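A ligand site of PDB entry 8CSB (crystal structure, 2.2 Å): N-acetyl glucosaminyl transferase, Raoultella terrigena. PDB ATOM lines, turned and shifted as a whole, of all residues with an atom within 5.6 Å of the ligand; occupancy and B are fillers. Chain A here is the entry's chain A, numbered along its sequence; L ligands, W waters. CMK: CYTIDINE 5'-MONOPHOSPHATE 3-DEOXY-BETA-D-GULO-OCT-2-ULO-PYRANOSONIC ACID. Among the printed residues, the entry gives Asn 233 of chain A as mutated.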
ATOM      1  N   GLU A 159       0.741   7.445 -11.138  1.00  0.00           N
ATOM      2  CA  GLU A 159       1.830   6.827 -11.873  1.00  0.00           C
ATOM      3  C   GLU A 159       1.657   5.344 -11.673  1.00  0.00           C
ATOM      4  O   GLU A 159       0.985   4.912 -10.737  1.00  0.00           O
ATOM      5  CB  GLU A 159       3.205   7.329 -11.332  1.00  0.00           C
ATOM      6  CG  GLU A 159       4.510   6.919 -12.004  1.00  0.00           C
ATOM      7  CD  GLU A 159       4.573   7.087 -13.537  1.00  0.00           C
ATOM      8  OE1 GLU A 159       3.784   6.446 -14.268  1.00  0.00           O
ATOM      9  OE2 GLU A 159       5.454   7.809 -14.036  1.00  0.00           O
ATOM     10  N   ILE A 160       2.230   4.556 -12.617  1.00  0.00           N
ATOM     11  CA  ILE A 160       2.305   3.119 -12.410  1.00  0.00           C
ATOM     12  C   ILE A 160       3.062   2.818 -11.110  1.00  0.00           C
ATOM     13  O   ILE A 160       4.018   3.527 -10.719  1.00  0.00           O
ATOM     14  CB  ILE A 160       2.966   2.416 -13.605  1.00  0.00           C
ATOM     15  CG1 ILE A 160       2.750   0.889 -13.471  1.00  0.00           C
ATOM     16  CG2 ILE A 160       4.478   2.765 -13.751  1.00  0.00           C
ATOM     17  CD1 ILE A 160       2.950   0.100 -14.757  1.00  0.00           C
ATOM     18  N   GLY A 161       2.594   1.752 -10.417  1.00  0.00           N
ATOM     19  CA  GLY A 161       3.101   1.417  -9.105  1.00  0.00           C
ATOM     20  C   GLY A 161       4.438   0.691  -9.146  1.00  0.00           C
ATOM     21  O   GLY A 161       5.014   0.447 -10.215  1.00  0.00           O
ATOM     22  N   PRO A 162       4.966   0.343  -7.959  1.00  0.00           N
ATOM     23  CA  PRO A 162       6.208  -0.448  -7.916  1.00  0.00           C
ATOM     24  C   PRO A 162       5.989  -1.964  -8.098  1.00  0.00           C
ATOM     25  O   PRO A 162       6.980  -2.673  -8.336  1.00  0.00           O
ATOM     26  CB  PRO A 162       6.766  -0.135  -6.527  1.00  0.00           C
ATOM     27  CG  PRO A 162       5.429   0.141  -5.633  1.00  0.00           C
ATOM     28  CD  PRO A 162       4.339   0.548  -6.633  1.00  0.00           C
ATOM     29  N   ARG A 164       4.070  -4.749 -10.562  1.00  0.00           N
ATOM     30  CA  ARG A 164       3.542  -4.702 -11.931  1.00  0.00           C
ATOM     31  C   ARG A 164       3.373  -6.099 -12.534  1.00  0.00           C
ATOM     32  O   ARG A 164       4.114  -7.023 -12.198  1.00  0.00           O
ATOM     33  CB  ARG A 164       4.474  -3.887 -12.844  1.00  0.00           C
ATOM     34  CG  ARG A 164       4.795  -2.475 -12.259  1.00  0.00           C
ATOM     35  CD  ARG A 164       5.855  -1.760 -13.088  1.00  0.00           C
ATOM     36  NE  ARG A 164       6.316  -0.514 -12.519  1.00  0.00           N
ATOM     37  CZ  ARG A 164       7.260   0.231 -13.060  1.00  0.00           C
ATOM     38  NH1 ARG A 164       7.867  -0.132 -14.180  1.00  0.00           N
ATOM     39  NH2 ARG A 164       7.595   1.374 -12.481  1.00  0.00           N
ATOM     40  N   TYR A 173       0.265   4.379  -8.128  1.00  0.00           N
ATOM     41  CA  TYR A 173       0.364   5.381  -7.069  1.00  0.00           C
ATOM     42  C   TYR A 173      -0.780   6.372  -7.204  1.00  0.00           C
ATOM     43  O   TYR A 173      -1.211   6.672  -8.321  1.00  0.00           O
ATOM     44  CB  TYR A 173       1.658   6.164  -7.149  1.00  0.00           C
ATOM     45  CG  TYR A 173       2.915   5.404  -6.834  1.00  0.00           C
ATOM     46  CD1 TYR A 173       3.141   4.935  -5.564  1.00  0.00           C
ATOM     47  CD2 TYR A 173       3.911   5.246  -7.801  1.00  0.00           C
ATOM     48  CE1 TYR A 173       4.311   4.304  -5.242  1.00  0.00           C
ATOM     49  CE2 TYR A 173       5.104   4.596  -7.502  1.00  0.00           C
ATOM     50  CZ  TYR A 173       5.297   4.127  -6.198  1.00  0.00           C
ATOM     51  OH  TYR A 173       6.446   3.445  -5.838  1.00  0.00           O
ATOM     52  N   VAL A 179       4.198  12.243  -6.240  1.00  0.00           N
ATOM     53  CA  VAL A 179       4.456  10.873  -6.684  1.00  0.00           C
ATOM     54  C   VAL A 179       5.968  10.701  -6.762  1.00  0.00           C
ATOM     55  O   VAL A 179       6.674  11.570  -7.294  1.00  0.00           O
ATOM     56  CB  VAL A 179       3.752  10.592  -8.035  1.00  0.00           C
ATOM     57  CG1 VAL A 179       4.281  11.523  -9.122  1.00  0.00           C
ATOM     58  CG2 VAL A 179       3.813   9.099  -8.450  1.00  0.00           C
ATOM     59  N   ASN A 180       6.482   9.621  -6.145  1.00  0.00           N
ATOM     60  CA  ASN A 180       7.928   9.388  -5.992  1.00  0.00           C
ATOM     61  C   ASN A 180       8.631  10.326  -5.014  1.00  0.00           C
ATOM     62  O   ASN A 180       9.167   9.874  -3.978  1.00  0.00           O
ATOM     63  CB  ASN A 180       8.615   9.459  -7.364  1.00  0.00           C
ATOM     64  CG  ASN A 180       8.206   8.301  -8.230  1.00  0.00           C
ATOM     65  OD1 ASN A 180       7.996   7.211  -7.718  1.00  0.00           O
ATOM     66  ND2 ASN A 180       8.044   8.542  -9.525  1.00  0.00           N
ATOM     67  N   VAL A 227      21.308  -2.427  -7.400  1.00  0.00           N
ATOM     68  CA  VAL A 227      20.222  -2.192  -8.355  1.00  0.00           C
ATOM     69  C   VAL A 227      20.530  -0.945  -9.153  1.00  0.00           C
ATOM     70  O   VAL A 227      20.576   0.146  -8.576  1.00  0.00           O
ATOM     71  CB  VAL A 227      18.876  -1.982  -7.659  1.00  0.00           C
ATOM     72  CG1 VAL A 227      17.830  -1.552  -8.724  1.00  0.00           C
ATOM     73  CG2 VAL A 227      18.466  -3.248  -6.831  1.00  0.00           C
ATOM     74  N   LEU A 228      20.619  -1.055 -10.472  1.00  0.00           N
ATOM     75  CA  LEU A 228      20.796   0.161 -11.261  1.00  0.00           C
ATOM     76  C   LEU A 228      19.435   0.598 -11.814  1.00  0.00           C
ATOM     77  O   LEU A 228      18.495  -0.190 -11.873  1.00  0.00           O
ATOM     78  CB  LEU A 228      21.837  -0.061 -12.362  1.00  0.00           C
ATOM     79  CG  LEU A 228      23.211  -0.604 -11.901  1.00  0.00           C
ATOM     80  CD1 LEU A 228      24.257  -0.523 -13.009  1.00  0.00           C
ATOM     81  CD2 LEU A 228      23.677   0.119 -10.609  1.00  0.00           C
ATOM     82  N   GLN A 229      19.318   1.897 -12.148  1.00  0.00           N
ATOM     83  CA  GLN A 229      18.054   2.430 -12.610  1.00  0.00           C
ATOM     84  C   GLN A 229      18.239   3.081 -13.967  1.00  0.00           C
ATOM     85  O   GLN A 229      19.357   3.244 -14.446  1.00  0.00           O
ATOM     86  CB  GLN A 229      17.484   3.456 -11.607  1.00  0.00           C
ATOM     87  CG  GLN A 229      17.067   2.759 -10.328  1.00  0.00           C
ATOM     88  CD  GLN A 229      16.540   3.734  -9.332  1.00  0.00           C
ATOM     89  OE1 GLN A 229      17.135   3.896  -8.278  1.00  0.00           O
ATOM     90  NE2 GLN A 229      15.409   4.403  -9.651  1.00  0.00           N
ATOM     91  N   VAL A 230      17.128   3.460 -14.592  1.00  0.00           N
ATOM     92  CA  VAL A 230      17.245   4.238 -15.823  1.00  0.00           C
ATOM     93  C   VAL A 230      17.833   5.605 -15.516  1.00  0.00           C
ATOM     94  O   VAL A 230      17.434   6.281 -14.551  1.00  0.00           O
ATOM     95  CB  VAL A 230      15.918   4.334 -16.583  1.00  0.00           C
ATOM     96  CG1 VAL A 230      16.165   5.035 -17.988  1.00  0.00           C
ATOM     97  CG2 VAL A 230      15.343   2.865 -16.861  1.00  0.00           C
ATOM     98  N   ASN A 233      15.591   8.771 -15.614  1.00  0.00           N
ATOM     99  CA  ASN A 233      14.268   8.678 -15.018  1.00  0.00           C
ATOM    100  C   ASN A 233      14.053   9.814 -13.997  1.00  0.00           C
ATOM    101  O   ASN A 233      14.988  10.249 -13.331  1.00  0.00           O
ATOM    102  CB  ASN A 233      14.118   7.314 -14.347  1.00  0.00           C
ATOM    103  CG  ASN A 233      12.679   6.975 -13.999  1.00  0.00           C
ATOM    104  OD1 ASN A 233      12.217   7.176 -12.845  1.00  0.00           O
ATOM    105  ND2 ASN A 233      11.934   6.490 -14.984  1.00  0.00           N
ATOM    106  N   SER A 234      12.792  10.293 -13.873  1.00  0.00           N
ATOM    107  CA  SER A 234      12.464  11.355 -12.906  1.00  0.00           C
ATOM    108  C   SER A 234      13.042  11.061 -11.515  1.00  0.00           C
ATOM    109  O   SER A 234      13.671  11.941 -10.924  1.00  0.00           O
ATOM    110  CB  SER A 234      10.941  11.579 -12.854  1.00  0.00           C
ATOM    111  OG  SER A 234      10.225  10.531 -12.212  1.00  0.00           O
ATOM    112  N   ASN A 235      12.924   9.800 -11.038  1.00  0.00           N
ATOM    113  CA  ASN A 235      13.558   9.284  -9.812  1.00  0.00           C
ATOM    114  C   ASN A 235      15.051   9.581  -9.695  1.00  0.00           C
ATOM    115  O   ASN A 235      15.555   9.840  -8.582  1.00  0.00           O
ATOM    116  CB  ASN A 235      13.420   7.756  -9.758  1.00  0.00           C
ATOM    117  CG  ASN A 235      12.130   7.317  -9.229  1.00  0.00           C
ATOM    118  OD1 ASN A 235      11.157   8.069  -9.224  1.00  0.00           O
ATOM    119  ND2 ASN A 235      12.071   6.087  -8.753  1.00  0.00           N
ATOM    120  N   LEU A 236      15.786   9.417 -10.787  1.00  0.00           N
ATOM    121  CA  LEU A 236      17.235   9.657 -10.829  1.00  0.00           C
ATOM    122  C   LEU A 236      17.632  11.098 -11.151  1.00  0.00           C
ATOM    123  O   LEU A 236      18.822  11.447 -11.052  1.00  0.00           O
ATOM    124  CB  LEU A 236      17.883   8.715 -11.856  1.00  0.00           C
ATOM    125  CG  LEU A 236      18.860   7.894 -11.048  1.00  0.00           C
ATOM    126  CD1 LEU A 236      18.022   7.036 -10.145  1.00  0.00           C
ATOM    127  CD2 LEU A 236      19.656   7.088 -12.003  1.00  0.00           C
ATOM    128  N   ARG A 264      22.820  -5.648 -11.167  1.00  0.00           N
ATOM    129  CA  ARG A 264      21.756  -5.777 -12.165  1.00  0.00           C
ATOM    130  C   ARG A 264      21.482  -4.408 -12.820  1.00  0.00           C
ATOM    131  O   ARG A 264      20.910  -3.505 -12.184  1.00  0.00           O
ATOM    132  CB  ARG A 264      20.485  -6.347 -11.541  1.00  0.00           C
ATOM    133  CG  ARG A 264      19.353  -6.468 -12.562  1.00  0.00           C
ATOM    134  CD  ARG A 264      18.160  -7.236 -12.026  1.00  0.00           C
ATOM    135  NE  ARG A 264      17.035  -7.263 -12.950  1.00  0.00           N
ATOM    136  CZ  ARG A 264      16.841  -8.178 -13.898  1.00  0.00           C
ATOM    137  NH1 ARG A 264      17.713  -9.167 -14.109  1.00  0.00           N
ATOM    138  NH2 ARG A 264      15.759  -8.101 -14.681  1.00  0.00           N
ATOM    139  N   ALA A 265      21.876  -4.272 -14.083  1.00  0.00           N
ATOM    140  CA  ALA A 265      21.426  -3.150 -14.883  1.00  0.00           C
ATOM    141  C   ALA A 265      19.900  -3.169 -15.013  1.00  0.00           C
ATOM    142  O   ALA A 265      19.246  -4.220 -14.857  1.00  0.00           O
ATOM    143  CB  ALA A 265      22.107  -3.186 -16.241  1.00  0.00           C
ATOM    144  N   HIS A 266      19.304  -1.971 -15.212  1.00  0.00           N
ATOM    145  CA  HIS A 266      17.868  -1.861 -15.527  1.00  0.00           C
ATOM    146  C   HIS A 266      17.654  -2.320 -16.968  1.00  0.00           C
ATOM    147  O   HIS A 266      18.265  -1.750 -17.866  1.00  0.00           O
ATOM    148  CB  HIS A 266      17.357  -0.378 -15.358  1.00  0.00           C
ATOM    149  CG  HIS A 266      15.848  -0.234 -15.310  1.00  0.00           C
ATOM    150  ND1 HIS A 266      15.030  -0.483 -16.396  1.00  0.00           N
ATOM    151  CD2 HIS A 266      15.018   0.135 -14.293  1.00  0.00           C
ATOM    152  CE1 HIS A 266      13.764  -0.274 -16.055  1.00  0.00           C
ATOM    153  NE2 HIS A 266      13.736   0.102 -14.788  1.00  0.00           N
ATOM    154  N   PRO A 267      16.824  -3.345 -17.234  1.00  0.00           N
ATOM    155  CA  PRO A 267      16.501  -3.692 -18.644  1.00  0.00           C
ATOM    156  C   PRO A 267      16.152  -2.491 -19.496  1.00  0.00           C
ATOM    157  O   PRO A 267      16.472  -2.469 -20.668  1.00  0.00           O
ATOM    158  CB  PRO A 267      15.279  -4.618 -18.498  1.00  0.00           C
ATOM    159  CG  PRO A 267      15.467  -5.323 -17.239  1.00  0.00           C
ATOM    160  CD  PRO A 267      16.145  -4.253 -16.284  1.00  0.00           C
ATOM    161  N   ASN A 285      14.440 -11.823 -14.226  1.00  0.00           N
ATOM    162  CA  ASN A 285      13.533 -10.892 -13.577  1.00  0.00           C
ATOM    163  C   ASN A 285      14.139 -10.416 -12.248  1.00  0.00           C
ATOM    164  O   ASN A 285      15.007 -11.075 -11.673  1.00  0.00           O
ATOM    165  CB  ASN A 285      12.163 -11.553 -13.386  1.00  0.00           C
ATOM    166  CG  ASN A 285      12.227 -12.679 -12.419  1.00  0.00           C
ATOM    167  OD1 ASN A 285      12.475 -12.473 -11.211  1.00  0.00           O
ATOM    168  ND2 ASN A 285      11.968 -13.886 -12.903  1.00  0.00           N
ATOM    169  N   SER A 286      13.696  -9.252 -11.756  1.00  0.00           N
ATOM    170  CA  SER A 286      14.432  -8.687 -10.600  1.00  0.00           C
ATOM    171  C   SER A 286      14.264  -9.508  -9.329  1.00  0.00           C
ATOM    172  O   SER A 286      15.142  -9.491  -8.448  1.00  0.00           O
ATOM    173  CB  SER A 286      14.043  -7.226 -10.320  1.00  0.00           C
ATOM    174  OG  SER A 286      12.672  -7.079 -10.012  1.00  0.00           O
ATOM    175  N   ASN A 300      16.388   4.576  -5.481  1.00  0.00           N
ATOM    176  CA  ASN A 300      14.956   4.559  -5.188  1.00  0.00           C
ATOM    177  C   ASN A 300      14.151   3.745  -6.210  1.00  0.00           C
ATOM    178  O   ASN A 300      13.037   4.137  -6.576  1.00  0.00           O
ATOM    179  CB  ASN A 300      14.401   6.000  -5.072  1.00  0.00           C
ATOM    180  CG  ASN A 300      14.845   6.904  -6.204  1.00  0.00           C
ATOM    181  OD1 ASN A 300      15.241   6.413  -7.251  1.00  0.00           O
ATOM    182  ND2 ASN A 300      14.770   8.248  -6.006  1.00  0.00           N
ATOM    183  N   SER A 301      14.688   2.608  -6.654  1.00  0.00           N
ATOM    184  CA  SER A 301      14.042   1.770  -7.648  1.00  0.00           C
ATOM    185  C   SER A 301      12.882   0.981  -7.017  1.00  0.00           C
ATOM    186  O   SER A 301      12.929   0.637  -5.841  1.00  0.00           O
ATOM    187  CB  SER A 301      15.078   0.816  -8.258  1.00  0.00           C
ATOM    188  OG  SER A 301      14.517  -0.431  -8.713  1.00  0.00           O
ATOM    189  N   SER A 302      11.839   0.710  -7.808  1.00  0.00           N
ATOM    190  CA  SER A 302      10.791  -0.222  -7.346  1.00  0.00           C
ATOM    191  C   SER A 302      11.370  -1.494  -6.791  1.00  0.00           C
ATOM    192  O   SER A 302      10.789  -2.090  -5.884  1.00  0.00           O
ATOM    193  CB  SER A 302       9.829  -0.561  -8.463  1.00  0.00           C
ATOM    194  OG  SER A 302       9.420   0.630  -9.086  1.00  0.00           O
ATOM    195  N   VAL A 303      12.521  -1.944  -7.295  1.00  0.00           N
ATOM    196  CA  VAL A 303      13.060  -3.254  -6.838  1.00  0.00           C
ATOM    197  C   VAL A 303      13.413  -3.229  -5.348  1.00  0.00           C
ATOM    198  O   VAL A 303      13.431  -4.303  -4.694  1.00  0.00           O
ATOM    199  CB  VAL A 303      14.300  -3.686  -7.671  1.00  0.00           C
ATOM    200  CG1 VAL A 303      14.986  -4.893  -6.996  1.00  0.00           C
ATOM    201  CG2 VAL A 303      13.921  -3.894  -9.101  1.00  0.00           C
ATOM    202  N   GLU A 306      10.637  -4.710  -3.403  1.00  0.00           N
ATOM    203  CA  GLU A 306      10.725  -6.151  -3.579  1.00  0.00           C
ATOM    204  C   GLU A 306      11.738  -6.756  -2.617  1.00  0.00           C
ATOM    205  O   GLU A 306      11.469  -7.768  -1.938  1.00  0.00           O
ATOM    206  CB  GLU A 306      11.105  -6.367  -5.057  1.00  0.00           C
ATOM    207  CG  GLU A 306      10.780  -7.649  -5.678  1.00  0.00           C
ATOM    208  CD  GLU A 306      10.945  -7.664  -7.228  1.00  0.00           C
ATOM    209  OE1 GLU A 306      11.574  -6.736  -7.846  1.00  0.00           O
ATOM    210  OE2 GLU A 306      10.399  -8.603  -7.805  1.00  0.00           O
HETATM  211  N1C CMK L   1      13.863  -3.838 -12.788  1.00  0.00           N
HETATM  212  C2C CMK L   1      14.766  -4.837 -12.885  1.00  0.00           C
HETATM  213  N3C CMK L   1      16.064  -4.604 -12.569  1.00  0.00           N
HETATM  214  C4C CMK L   1      16.463  -3.395 -12.195  1.00  0.00           C
HETATM  215  C5C CMK L   1      15.570  -2.357 -12.120  1.00  0.00           C
HETATM  216  C6C CMK L   1      14.254  -2.607 -12.448  1.00  0.00           C
HETATM  217  O2C CMK L   1      14.466  -5.935 -13.194  1.00  0.00           O
HETATM  218  N4C CMK L   1      17.876  -3.240 -11.888  1.00  0.00           N
HETATM  219  C1' CMK L   1      12.600  -4.150 -13.105  1.00  0.00           C
HETATM  220  C2' CMK L   1      11.511  -4.490 -12.047  1.00  0.00           C
HETATM  221  O2' CMK L   1      10.546  -5.356 -12.826  1.00  0.00           O
HETATM  222  C3' CMK L   1      10.976  -3.334 -11.650  1.00  0.00           C
HETATM  223  C4' CMK L   1      11.032  -2.462 -13.038  1.00  0.00           C
HETATM  224  O4' CMK L   1      12.068  -2.846 -13.756  1.00  0.00           O
HETATM  225  O3' CMK L   1       9.649  -3.346 -11.050  1.00  0.00           O
HETATM  226  C5' CMK L   1      11.028  -0.984 -12.572  1.00  0.00           C
HETATM  227  O5' CMK L   1      11.896  -0.635 -11.429  1.00  0.00           O
HETATM  228  PA  CMK L   1      12.431   0.978 -11.346  1.00  0.00           P
HETATM  229  O1A CMK L   1      11.483   1.541 -10.353  1.00  0.00           O
HETATM  230  O2A CMK L   1      13.853   0.878 -10.882  1.00  0.00           O
HETATM  231  O6  CMK L   1      10.995   3.833 -12.092  1.00  0.00           O
HETATM  232  C2  CMK L   1      12.146   3.269 -12.884  1.00  0.00           C
HETATM  233  O2  CMK L   1      12.230   1.839 -12.779  1.00  0.00           O
HETATM  234  C3  CMK L   1      11.970   3.545 -14.384  1.00  0.00           C
HETATM  235  C4  CMK L   1      10.581   3.308 -14.802  1.00  0.00           C
HETATM  236  O4  CMK L   1      10.151   2.027 -14.307  1.00  0.00           O
HETATM  237  C5  CMK L   1       9.692   4.329 -14.177  1.00  0.00           C
HETATM  238  C6  CMK L   1      10.175   4.818 -12.834  1.00  0.00           C
HETATM  239  C7  CMK L   1       9.023   5.175 -11.925  1.00  0.00           C
HETATM  240  C1  CMK L   1      13.421   3.871 -12.403  1.00  0.00           C
HETATM  241  O1X CMK L   1      13.493   4.497 -11.266  1.00  0.00           O
HETATM  242  O1Y CMK L   1      14.413   3.666 -13.185  1.00  0.00           O
HETATM  243  O5  CMK L   1       8.421   3.692 -13.989  1.00  0.00           O
HETATM  244  C8  CMK L   1       8.678   6.667 -12.170  1.00  0.00           C
HETATM  245  O8  CMK L   1       7.377   6.926 -11.691  1.00  0.00           O
HETATM  246  O7  CMK L   1       7.935   4.292 -12.197  1.00  0.00           O
HETATM  247  O   HOH W   1      11.959  -8.150 -13.128  1.00  0.00           O
HETATM  248  O   HOH W   2       8.735  -6.804 -11.368  1.00  0.00           O
HETATM  249  O   HOH W   3       6.944  -5.017 -10.284  1.00  0.00           O
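The side-chain amide oxygen of Asn 233 sits close to an oxygen (O1X) of the ligand.
O of Ala 265 sits at hydrogen-bond distance from N4C of the ligand (3.4 Å).
ND2 of Asn 180 sits at hydrogen-bond distance from O8 of the ligand (2.8 Å).
N of Ser 302 is in hydrogen-bond range of O1A of the ligand.
The side-chain hydroxyl (OG) of Ser 302 sits at hydrogen-bond distance from an oxygen (O1A) of the ligand (2.6 Å).
The side-chain hydroxyl of Ser 301 sits at hydrogen-bond distance from an oxygen (O2A) of the ligand (2.6 Å).
ND2 of Asn 235 is in hydrogen-bond range of O1X of the ligand, 3.3 Å away.
OE2 of Glu 159 lies close to O8 of the ligand.
The guanidinium group (NE) of Arg 264 is in hydrogen-bond range of a nitrogen (N3C) of the ligand, at 2.9 Å.
O5 of the ligand is in hydrogen-bond range of NH2 of Arg 164 (2.9 Å).
O1Y of the ligand sits at hydrogen-bond distance from N of Val 230 (3.1 Å).
A ring nitrogen (NE2) of His 266 lies within hydrogen-bond range of an oxygen (O2) of the ligand.
O of Leu 228 sits at hydrogen-bond distance from N4C of the ligand.
The backbone carbonyl oxygen of Arg 264 lies within hydrogen-bond range of a nitrogen (N4C) of the ligand (3.1 Å).
The side-chain amide nitrogen (NE2) of Gln 229 is in hydrogen-bond range of an oxygen (O1X) of the ligand (2.5 Å).
The backbone carbonyl oxygen (O) of Gly 161 lies within hydrogen-bond range of the guanidinium group (NE) of Arg 164.
The backbone NH (N) of Asn 235 sits close to the side-chain amide oxygen (OD1) of Asn 233, 3.3 Å away.
OE1 of Glu 306 sits at hydrogen-bond distance from OG of Ser 286 (2.5 Å).
OG of Ser 301 is in hydrogen-bond range of N of Val 303, 2.9 Å away.
OE1 of Gln 229 sits at hydrogen-bond distance from N of Ser 301 (3.2 Å).
ND2 of Asn 235 lies within hydrogen-bond range of O of Asn 300, at 3.1 Å.
ND2 of Asn 180 sits close to OD1 of Asn 235 (3.2 Å).
O of Glu 159 sits at hydrogen-bond distance from N of Tyr 173, at 2.8 Å.
Residues that only touch the ligand: Pro 162 (3.9 Å), Val 227 (3.6 Å), Pro 267 (3.7 Å), Ser 286 (3.2 Å) and Val 303 (3.6 Å).
Hydrophobic or aromatic side chains within 4 Å of the ligand: Val 227, Val 230, His 266, Pro 267 and Val 303.
18 residues have an atom within 4 Å of the ligand: Glu 159, Pro 162, Arg 164, Asn 180, Val 227, Leu 228, Gln 229, Val 230, Asn 233, Asn 235, Arg 264, Ala 265, His 266, Pro 267, Ser 286, Ser 301, Ser 302 and Val 303.
Water W1 lies within hydrogen-bond range of the backbone NH of Ser 286 (2.5 Å) and an oxygen (O2') of the ligand (3.1 Å).
Water W3 lies within hydrogen-bond range of N of Arg 164, O of Pro 162 and O3' of the ligand.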
